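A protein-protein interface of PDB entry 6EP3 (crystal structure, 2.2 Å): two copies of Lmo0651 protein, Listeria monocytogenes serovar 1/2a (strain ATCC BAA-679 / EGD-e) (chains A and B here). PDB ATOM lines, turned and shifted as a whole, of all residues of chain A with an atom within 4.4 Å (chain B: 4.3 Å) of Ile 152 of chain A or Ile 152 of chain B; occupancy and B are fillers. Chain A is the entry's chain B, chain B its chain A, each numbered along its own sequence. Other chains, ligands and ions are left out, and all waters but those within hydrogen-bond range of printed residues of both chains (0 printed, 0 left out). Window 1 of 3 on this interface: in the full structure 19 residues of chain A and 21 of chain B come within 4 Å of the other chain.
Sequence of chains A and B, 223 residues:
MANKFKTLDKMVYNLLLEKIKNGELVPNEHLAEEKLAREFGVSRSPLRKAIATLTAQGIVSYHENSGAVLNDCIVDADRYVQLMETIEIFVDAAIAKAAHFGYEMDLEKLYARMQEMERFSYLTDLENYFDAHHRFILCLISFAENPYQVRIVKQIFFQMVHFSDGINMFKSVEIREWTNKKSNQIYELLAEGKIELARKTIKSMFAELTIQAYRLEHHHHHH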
ATOM      1  N   PHE A  90     -26.164  29.422   1.278  1.00  0.00           N
ATOM      2  CA  PHE A  90     -25.032  29.840   0.449  1.00  0.00           C
ATOM      3  C   PHE A  90     -24.765  31.344   0.565  1.00  0.00           C
ATOM      4  O   PHE A  90     -23.611  31.768   0.708  1.00  0.00           O
ATOM      5  CB  PHE A  90     -25.275  29.452  -1.007  1.00  0.00           C
ATOM      6  CG  PHE A  90     -24.855  28.050  -1.331  1.00  0.00           C
ATOM      7  CD1 PHE A  90     -23.626  27.569  -0.913  1.00  0.00           C
ATOM      8  CD2 PHE A  90     -25.688  27.213  -2.051  1.00  0.00           C
ATOM      9  CE1 PHE A  90     -23.237  26.276  -1.206  1.00  0.00           C
ATOM     10  CE2 PHE A  90     -25.303  25.920  -2.350  1.00  0.00           C
ATOM     11  CZ  PHE A  90     -24.076  25.451  -1.926  1.00  0.00           C
ATOM     12  N   TYR A 148     -17.797  26.826  -7.608  1.00  0.00           N
ATOM     13  CA  TYR A 148     -18.653  25.653  -7.446  1.00  0.00           C
ATOM     14  C   TYR A 148     -20.012  26.059  -6.893  1.00  0.00           C
ATOM     15  O   TYR A 148     -21.058  25.616  -7.386  1.00  0.00           O
ATOM     16  CB  TYR A 148     -17.986  24.623  -6.531  1.00  0.00           C
ATOM     17  CG  TYR A 148     -16.663  24.112  -7.050  1.00  0.00           C
ATOM     18  CD1 TYR A 148     -15.465  24.516  -6.474  1.00  0.00           C
ATOM     19  CD2 TYR A 148     -16.614  23.215  -8.107  1.00  0.00           C
ATOM     20  CE1 TYR A 148     -14.253  24.047  -6.947  1.00  0.00           C
ATOM     21  CE2 TYR A 148     -15.408  22.744  -8.589  1.00  0.00           C
ATOM     22  CZ  TYR A 148     -14.232  23.164  -8.004  1.00  0.00           C
ATOM     23  OH  TYR A 148     -13.033  22.697  -8.480  1.00  0.00           O
ATOM     24  N   GLN A 149     -20.011  26.918  -5.871  1.00  0.00           N
ATOM     25  CA  GLN A 149     -21.266  27.376  -5.291  1.00  0.00           C
ATOM     26  C   GLN A 149     -22.052  28.211  -6.287  1.00  0.00           C
ATOM     27  O   GLN A 149     -23.287  28.110  -6.354  1.00  0.00           O
ATOM     28  CB  GLN A 149     -20.998  28.171  -4.015  1.00  0.00           C
ATOM     29  CG  GLN A 149     -20.246  27.388  -2.945  1.00  0.00           C
ATOM     30  CD  GLN A 149     -19.989  28.215  -1.700  1.00  0.00           C
ATOM     31  OE1 GLN A 149     -20.151  29.437  -1.710  1.00  0.00           O
ATOM     32  NE2 GLN A 149     -19.599  27.552  -0.613  1.00  0.00           N
ATOM     33  N   VAL A 150     -21.357  29.039  -7.073  1.00  0.00           N
ATOM     34  CA  VAL A 150     -22.058  29.822  -8.091  1.00  0.00           C
ATOM     35  C   VAL A 150     -22.761  28.905  -9.091  1.00  0.00           C
ATOM     36  O   VAL A 150     -23.931  29.118  -9.432  1.00  0.00           O
ATOM     37  CB  VAL A 150     -21.090  30.793  -8.791  1.00  0.00           C
ATOM     38  CG1 VAL A 150     -21.778  31.470  -9.977  1.00  0.00           C
ATOM     39  CG2 VAL A 150     -20.573  31.830  -7.804  1.00  0.00           C
ATOM     40  N   ARG A 151     -22.072  27.860  -9.559  1.00  0.00           N
ATOM     41  CA  ARG A 151     -22.674  26.948 -10.532  1.00  0.00           C
ATOM     42  C   ARG A 151     -23.844  26.180  -9.926  1.00  0.00           C
ATOM     43  O   ARG A 151     -24.863  25.948 -10.593  1.00  0.00           O
ATOM     44  CB  ARG A 151     -21.629  25.966 -11.062  1.00  0.00           C
ATOM     45  CG  ARG A 151     -20.496  26.591 -11.859  1.00  0.00           C
ATOM     46  CD  ARG A 151     -19.553  25.512 -12.383  1.00  0.00           C
ATOM     47  NE  ARG A 151     -18.353  25.367 -11.562  1.00  0.00           N
ATOM     48  CZ  ARG A 151     -17.253  26.098 -11.693  1.00  0.00           C
ATOM     49  NH1 ARG A 151     -17.188  27.040 -12.621  1.00  0.00           N
ATOM     50  NH2 ARG A 151     -16.216  25.884 -10.894  1.00  0.00           N
ATOM     51  N   ILE A 152     -23.710  25.761  -8.666  1.00  0.00           N
ATOM     52  CA  ILE A 152     -24.806  25.066  -7.993  1.00  0.00           C
ATOM     53  C   ILE A 152     -26.044  25.954  -7.944  1.00  0.00           C
ATOM     54  O   ILE A 152     -27.159  25.530  -8.286  1.00  0.00           O
ATOM     55  CB  ILE A 152     -24.370  24.629  -6.583  1.00  0.00           C
ATOM     56  CG1 ILE A 152     -23.394  23.453  -6.660  1.00  0.00           C
ATOM     57  CG2 ILE A 152     -25.577  24.296  -5.716  1.00  0.00           C
ATOM     58  CD1 ILE A 152     -22.589  23.259  -5.390  1.00  0.00           C
ATOM     59  N   VAL A 153     -25.866  27.207  -7.525  1.00  0.00           N
ATOM     60  CA  VAL A 153     -27.019  28.091  -7.414  1.00  0.00           C
ATOM     61  C   VAL A 153     -27.564  28.456  -8.788  1.00  0.00           C
ATOM     62  O   VAL A 153     -28.768  28.680  -8.941  1.00  0.00           O
ATOM     63  CB  VAL A 153     -26.653  29.331  -6.585  1.00  0.00           C
ATOM     64  CG1 VAL A 153     -27.859  30.237  -6.423  1.00  0.00           C
ATOM     65  CG2 VAL A 153     -26.143  28.885  -5.225  1.00  0.00           C
ATOM     66  N   LYS A 154     -26.713  28.481  -9.816  1.00  0.00           N
ATOM     67  CA  LYS A 154     -27.217  28.683 -11.173  1.00  0.00           C
ATOM     68  C   LYS A 154     -28.123  27.533 -11.592  1.00  0.00           C
ATOM     69  O   LYS A 154     -29.174  27.749 -12.211  1.00  0.00           O
ATOM     70  CB  LYS A 154     -26.057  28.829 -12.156  1.00  0.00           C
ATOM     71  CG  LYS A 154     -25.446  30.223 -12.221  1.00  0.00           C
ATOM     72  CD  LYS A 154     -24.329  30.277 -13.257  1.00  0.00           C
ATOM     73  CE  LYS A 154     -23.796  31.692 -13.436  1.00  0.00           C
ATOM     74  NZ  LYS A 154     -22.662  31.752 -14.404  1.00  0.00           N
ATOM     75  N   GLN A 155     -27.727  26.302 -11.263  1.00  0.00           N
ATOM     76  CA  GLN A 155     -28.569  25.149 -11.571  1.00  0.00           C
ATOM     77  C   GLN A 155     -29.898  25.232 -10.823  1.00  0.00           C
ATOM     78  O   GLN A 155     -30.965  24.924 -11.376  1.00  0.00           O
ATOM     79  CB  GLN A 155     -27.836  23.856 -11.208  1.00  0.00           C
ATOM     80  CG  GLN A 155     -27.074  23.244 -12.365  1.00  0.00           C
ATOM     81  CD  GLN A 155     -27.974  22.783 -13.489  1.00  0.00           C
ATOM     82  OE1 GLN A 155     -27.621  22.898 -14.662  1.00  0.00           O
ATOM     83  NE2 GLN A 155     -29.145  22.261 -13.139  1.00  0.00           N
ATOM     84  N   ILE A 156     -29.844  25.653  -9.558  1.00  0.00           N
ATOM     85  CA  ILE A 156     -31.068  25.845  -8.779  1.00  0.00           C
ATOM     86  C   ILE A 156     -31.970  26.884  -9.437  1.00  0.00           C
ATOM     87  O   ILE A 156     -33.193  26.705  -9.524  1.00  0.00           O
ATOM     88  CB  ILE A 156     -30.729  26.250  -7.336  1.00  0.00           C
ATOM     89  CG1 ILE A 156     -30.151  25.068  -6.561  1.00  0.00           C
ATOM     90  CG2 ILE A 156     -31.963  26.814  -6.644  1.00  0.00           C
ATOM     91  CD1 ILE A 156     -29.801  25.427  -5.141  1.00  0.00           C
ATOM     92  N   PHE B  90     -23.401  22.780   4.205  1.00  0.00           N
ATOM     93  CA  PHE B  90     -24.590  21.929   4.144  1.00  0.00           C
ATOM     94  C   PHE B  90     -24.784  21.142   5.440  1.00  0.00           C
ATOM     95  O   PHE B  90     -25.898  21.067   5.969  1.00  0.00           O
ATOM     96  CB  PHE B  90     -24.492  20.980   2.953  1.00  0.00           C
ATOM     97  CG  PHE B  90     -24.974  21.575   1.671  1.00  0.00           C
ATOM     98  CD1 PHE B  90     -26.181  22.244   1.612  1.00  0.00           C
ATOM     99  CD2 PHE B  90     -24.200  21.495   0.526  1.00  0.00           C
ATOM    100  CE1 PHE B  90     -26.617  22.807   0.428  1.00  0.00           C
ATOM    101  CE2 PHE B  90     -24.630  22.053  -0.662  1.00  0.00           C
ATOM    102  CZ  PHE B  90     -25.840  22.711  -0.712  1.00  0.00           C
ATOM    103  N   TYR B 148     -32.451  17.737  -2.524  1.00  0.00           N
ATOM    104  CA  TYR B 148     -31.619  18.503  -3.449  1.00  0.00           C
ATOM    105  C   TYR B 148     -30.197  18.640  -2.928  1.00  0.00           C
ATOM    106  O   TYR B 148     -29.228  18.481  -3.683  1.00  0.00           O
ATOM    107  CB  TYR B 148     -32.214  19.893  -3.675  1.00  0.00           C
ATOM    108  CG  TYR B 148     -33.594  19.922  -4.287  1.00  0.00           C
ATOM    109  CD1 TYR B 148     -34.708  20.214  -3.511  1.00  0.00           C
ATOM    110  CD2 TYR B 148     -33.783  19.684  -5.643  1.00  0.00           C
ATOM    111  CE1 TYR B 148     -35.973  20.259  -4.064  1.00  0.00           C
ATOM    112  CE2 TYR B 148     -35.047  19.726  -6.208  1.00  0.00           C
ATOM    113  CZ  TYR B 148     -36.136  20.014  -5.413  1.00  0.00           C
ATOM    114  OH  TYR B 148     -37.394  20.055  -5.965  1.00  0.00           O
ATOM    115  N   GLN B 149     -30.054  18.951  -1.639  1.00  0.00           N
ATOM    116  CA  GLN B 149     -28.727  19.100  -1.059  1.00  0.00           C
ATOM    117  C   GLN B 149     -27.976  17.783  -1.074  1.00  0.00           C
ATOM    118  O   GLN B 149     -26.763  17.757  -1.316  1.00  0.00           O
ATOM    119  CB  GLN B 149     -28.840  19.635   0.364  1.00  0.00           C
ATOM    120  CG  GLN B 149     -29.570  20.958   0.433  1.00  0.00           C
ATOM    121  CD  GLN B 149     -29.677  21.476   1.842  1.00  0.00           C
ATOM    122  OE1 GLN B 149     -29.471  20.737   2.804  1.00  0.00           O
ATOM    123  NE2 GLN B 149     -30.004  22.750   1.976  1.00  0.00           N
ATOM    124  N   VAL B 150     -28.683  16.681  -0.824  1.00  0.00           N
ATOM    125  CA  VAL B 150     -28.044  15.372  -0.888  1.00  0.00           C
ATOM    126  C   VAL B 150     -27.487  15.131  -2.282  1.00  0.00           C
ATOM    127  O   VAL B 150     -26.344  14.691  -2.437  1.00  0.00           O
ATOM    128  CB  VAL B 150     -29.030  14.268  -0.463  1.00  0.00           C
ATOM    129  CG1 VAL B 150     -28.425  12.890  -0.716  1.00  0.00           C
ATOM    130  CG2 VAL B 150     -29.406  14.431   1.007  1.00  0.00           C
ATOM    131  N   ARG B 151     -28.268  15.450  -3.319  1.00  0.00           N
ATOM    132  CA  ARG B 151     -27.788  15.244  -4.685  1.00  0.00           C
ATOM    133  C   ARG B 151     -26.605  16.149  -5.010  1.00  0.00           C
ATOM    134  O   ARG B 151     -25.644  15.722  -5.667  1.00  0.00           O
ATOM    135  CB  ARG B 151     -28.931  15.467  -5.674  1.00  0.00           C
ATOM    136  CG  ARG B 151     -30.005  14.408  -5.576  1.00  0.00           C
ATOM    137  CD  ARG B 151     -31.135  14.641  -6.550  1.00  0.00           C
ATOM    138  NE  ARG B 151     -32.300  15.201  -5.873  1.00  0.00           N
ATOM    139  CZ  ARG B 151     -33.223  15.951  -6.462  1.00  0.00           C
ATOM    140  NH1 ARG B 151     -33.120  16.239  -7.752  1.00  0.00           N
ATOM    141  NH2 ARG B 151     -34.251  16.409  -5.759  1.00  0.00           N
ATOM    142  N   ILE B 152     -26.652  17.399  -4.552  1.00  0.00           N
ATOM    143  CA  ILE B 152     -25.539  18.316  -4.778  1.00  0.00           C
ATOM    144  C   ILE B 152     -24.258  17.763  -4.162  1.00  0.00           C
ATOM    145  O   ILE B 152     -23.211  17.668  -4.822  1.00  0.00           O
ATOM    146  CB  ILE B 152     -25.886  19.706  -4.216  1.00  0.00           C
ATOM    147  CG1 ILE B 152     -26.908  20.402  -5.123  1.00  0.00           C
ATOM    148  CG2 ILE B 152     -24.628  20.533  -3.994  1.00  0.00           C
ATOM    149  CD1 ILE B 152     -27.653  21.544  -4.458  1.00  0.00           C
ATOM    150  N   VAL B 153     -24.334  17.349  -2.899  1.00  0.00           N
ATOM    151  CA  VAL B 153     -23.139  16.846  -2.230  1.00  0.00           C
ATOM    152  C   VAL B 153     -22.710  15.508  -2.817  1.00  0.00           C
ATOM    153  O   VAL B 153     -21.519  15.179  -2.813  1.00  0.00           O
ATOM    154  CB  VAL B 153     -23.383  16.775  -0.716  1.00  0.00           C
ATOM    155  CG1 VAL B 153     -22.139  16.294   0.013  1.00  0.00           C
ATOM    156  CG2 VAL B 153     -23.769  18.152  -0.224  1.00  0.00           C
ATOM    157  N   LYS B 154     -23.649  14.735  -3.370  1.00  0.00           N
ATOM    158  CA  LYS B 154     -23.269  13.525  -4.093  1.00  0.00           C
ATOM    159  C   LYS B 154     -22.423  13.866  -5.314  1.00  0.00           C
ATOM    160  O   LYS B 154     -21.420  13.195  -5.591  1.00  0.00           O
ATOM    161  CB  LYS B 154     -24.517  12.744  -4.509  1.00  0.00           C
ATOM    162  CG  LYS B 154     -25.120  11.872  -3.416  1.00  0.00           C
ATOM    163  CD  LYS B 154     -26.336  11.100  -3.932  1.00  0.00           C
ATOM    164  CE  LYS B 154     -26.860  10.120  -2.886  1.00  0.00           C
ATOM    165  NZ  LYS B 154     -28.081   9.392  -3.338  1.00  0.00           N
ATOM    166  N   GLN B 155     -22.809  14.912  -6.055  1.00  0.00           N
ATOM    167  CA  GLN B 155     -21.984  15.351  -7.183  1.00  0.00           C
ATOM    168  C   GLN B 155     -20.612  15.819  -6.717  1.00  0.00           C
ATOM    169  O   GLN B 155     -19.591  15.529  -7.360  1.00  0.00           O
ATOM    170  CB  GLN B 155     -22.683  16.462  -7.968  1.00  0.00           C
ATOM    171  CG  GLN B 155     -23.337  15.979  -9.245  1.00  0.00           C
ATOM    172  CD  GLN B 155     -22.307  15.506 -10.263  1.00  0.00           C
ATOM    173  OE1 GLN B 155     -21.213  16.066 -10.363  1.00  0.00           O
ATOM    174  NE2 GLN B 155     -22.649  14.464 -11.016  1.00  0.00           N
ATOM    175  N   ILE B 156     -20.570  16.540  -5.597  1.00  0.00           N
ATOM    176  CA  ILE B 156     -19.287  16.976  -5.048  1.00  0.00           C
ATOM    177  C   ILE B 156     -18.404  15.777  -4.730  1.00  0.00           C
ATOM    178  O   ILE B 156     -17.217  15.744  -5.081  1.00  0.00           O
ATOM    179  CB  ILE B 156     -19.506  17.844  -3.801  1.00  0.00           C
ATOM    180  CG1 ILE B 156     -20.069  19.208  -4.204  1.00  0.00           C
ATOM    181  CG2 ILE B 156     -18.210  17.957  -3.007  1.00  0.00           C
ATOM    182  CD1 ILE B 156     -20.337  20.118  -3.024  1.00  0.00           C
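Of the printed residues of chain B, Phe 90 of chain A touches Phe 90 (3.5 Å). Tyr 148 of chain A touches none of the printed residues of chain B. Ile 152 of chain A touches just one residue of chain B: Ile 152. Lys 154 of chain A touches none of the printed residues of chain B. Printed residues of chain A within 4 Å of Phe 90 of chain B: Phe 90. Ile 152 of chain B touches one residue of chain A. The nearest printed residue of chain A that does not touch Ile 152 of chain B is Ile 156 of chain A (4.5 Å). The nearest printed residue of chain B that does not touch Phe 90 of chain A is Ile 152 of chain B (5.4 Å).
Of the 10 printed residues of chain B, 2 touch a printed residue of chain A. Hydrophobic or aromatic side chains of chain B within 4 Å of the printed part of chain A: Phe 90 and Ile 152. Of the 10 printed residues of chain A, 2 touch a printed residue of chain B. Printed residues of chain A that touch a printed residue of chain B: Phe 90 and Ile 152. Hydrophobic or aromatic side chains of chain A within 4 Å of the printed part of chain B: Phe 90 and Ile 152.
CZ of Phe 90 of chain B touches CZ of Phe 90 of chain A (3.5 Å). CG2 of Ile 152 of chain A touches CD1 of Ile 152 of chain B (3.7 Å).
Phe 90 of chain B touches its own counterpart, Phe 90 of chain A. Ile 152 of chain A touches its own counterpart, Ile 152 of chain B. Positions printed for both chains: 90, 148, 149, 150, 151, 152, 153, 154, 155 and 156.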
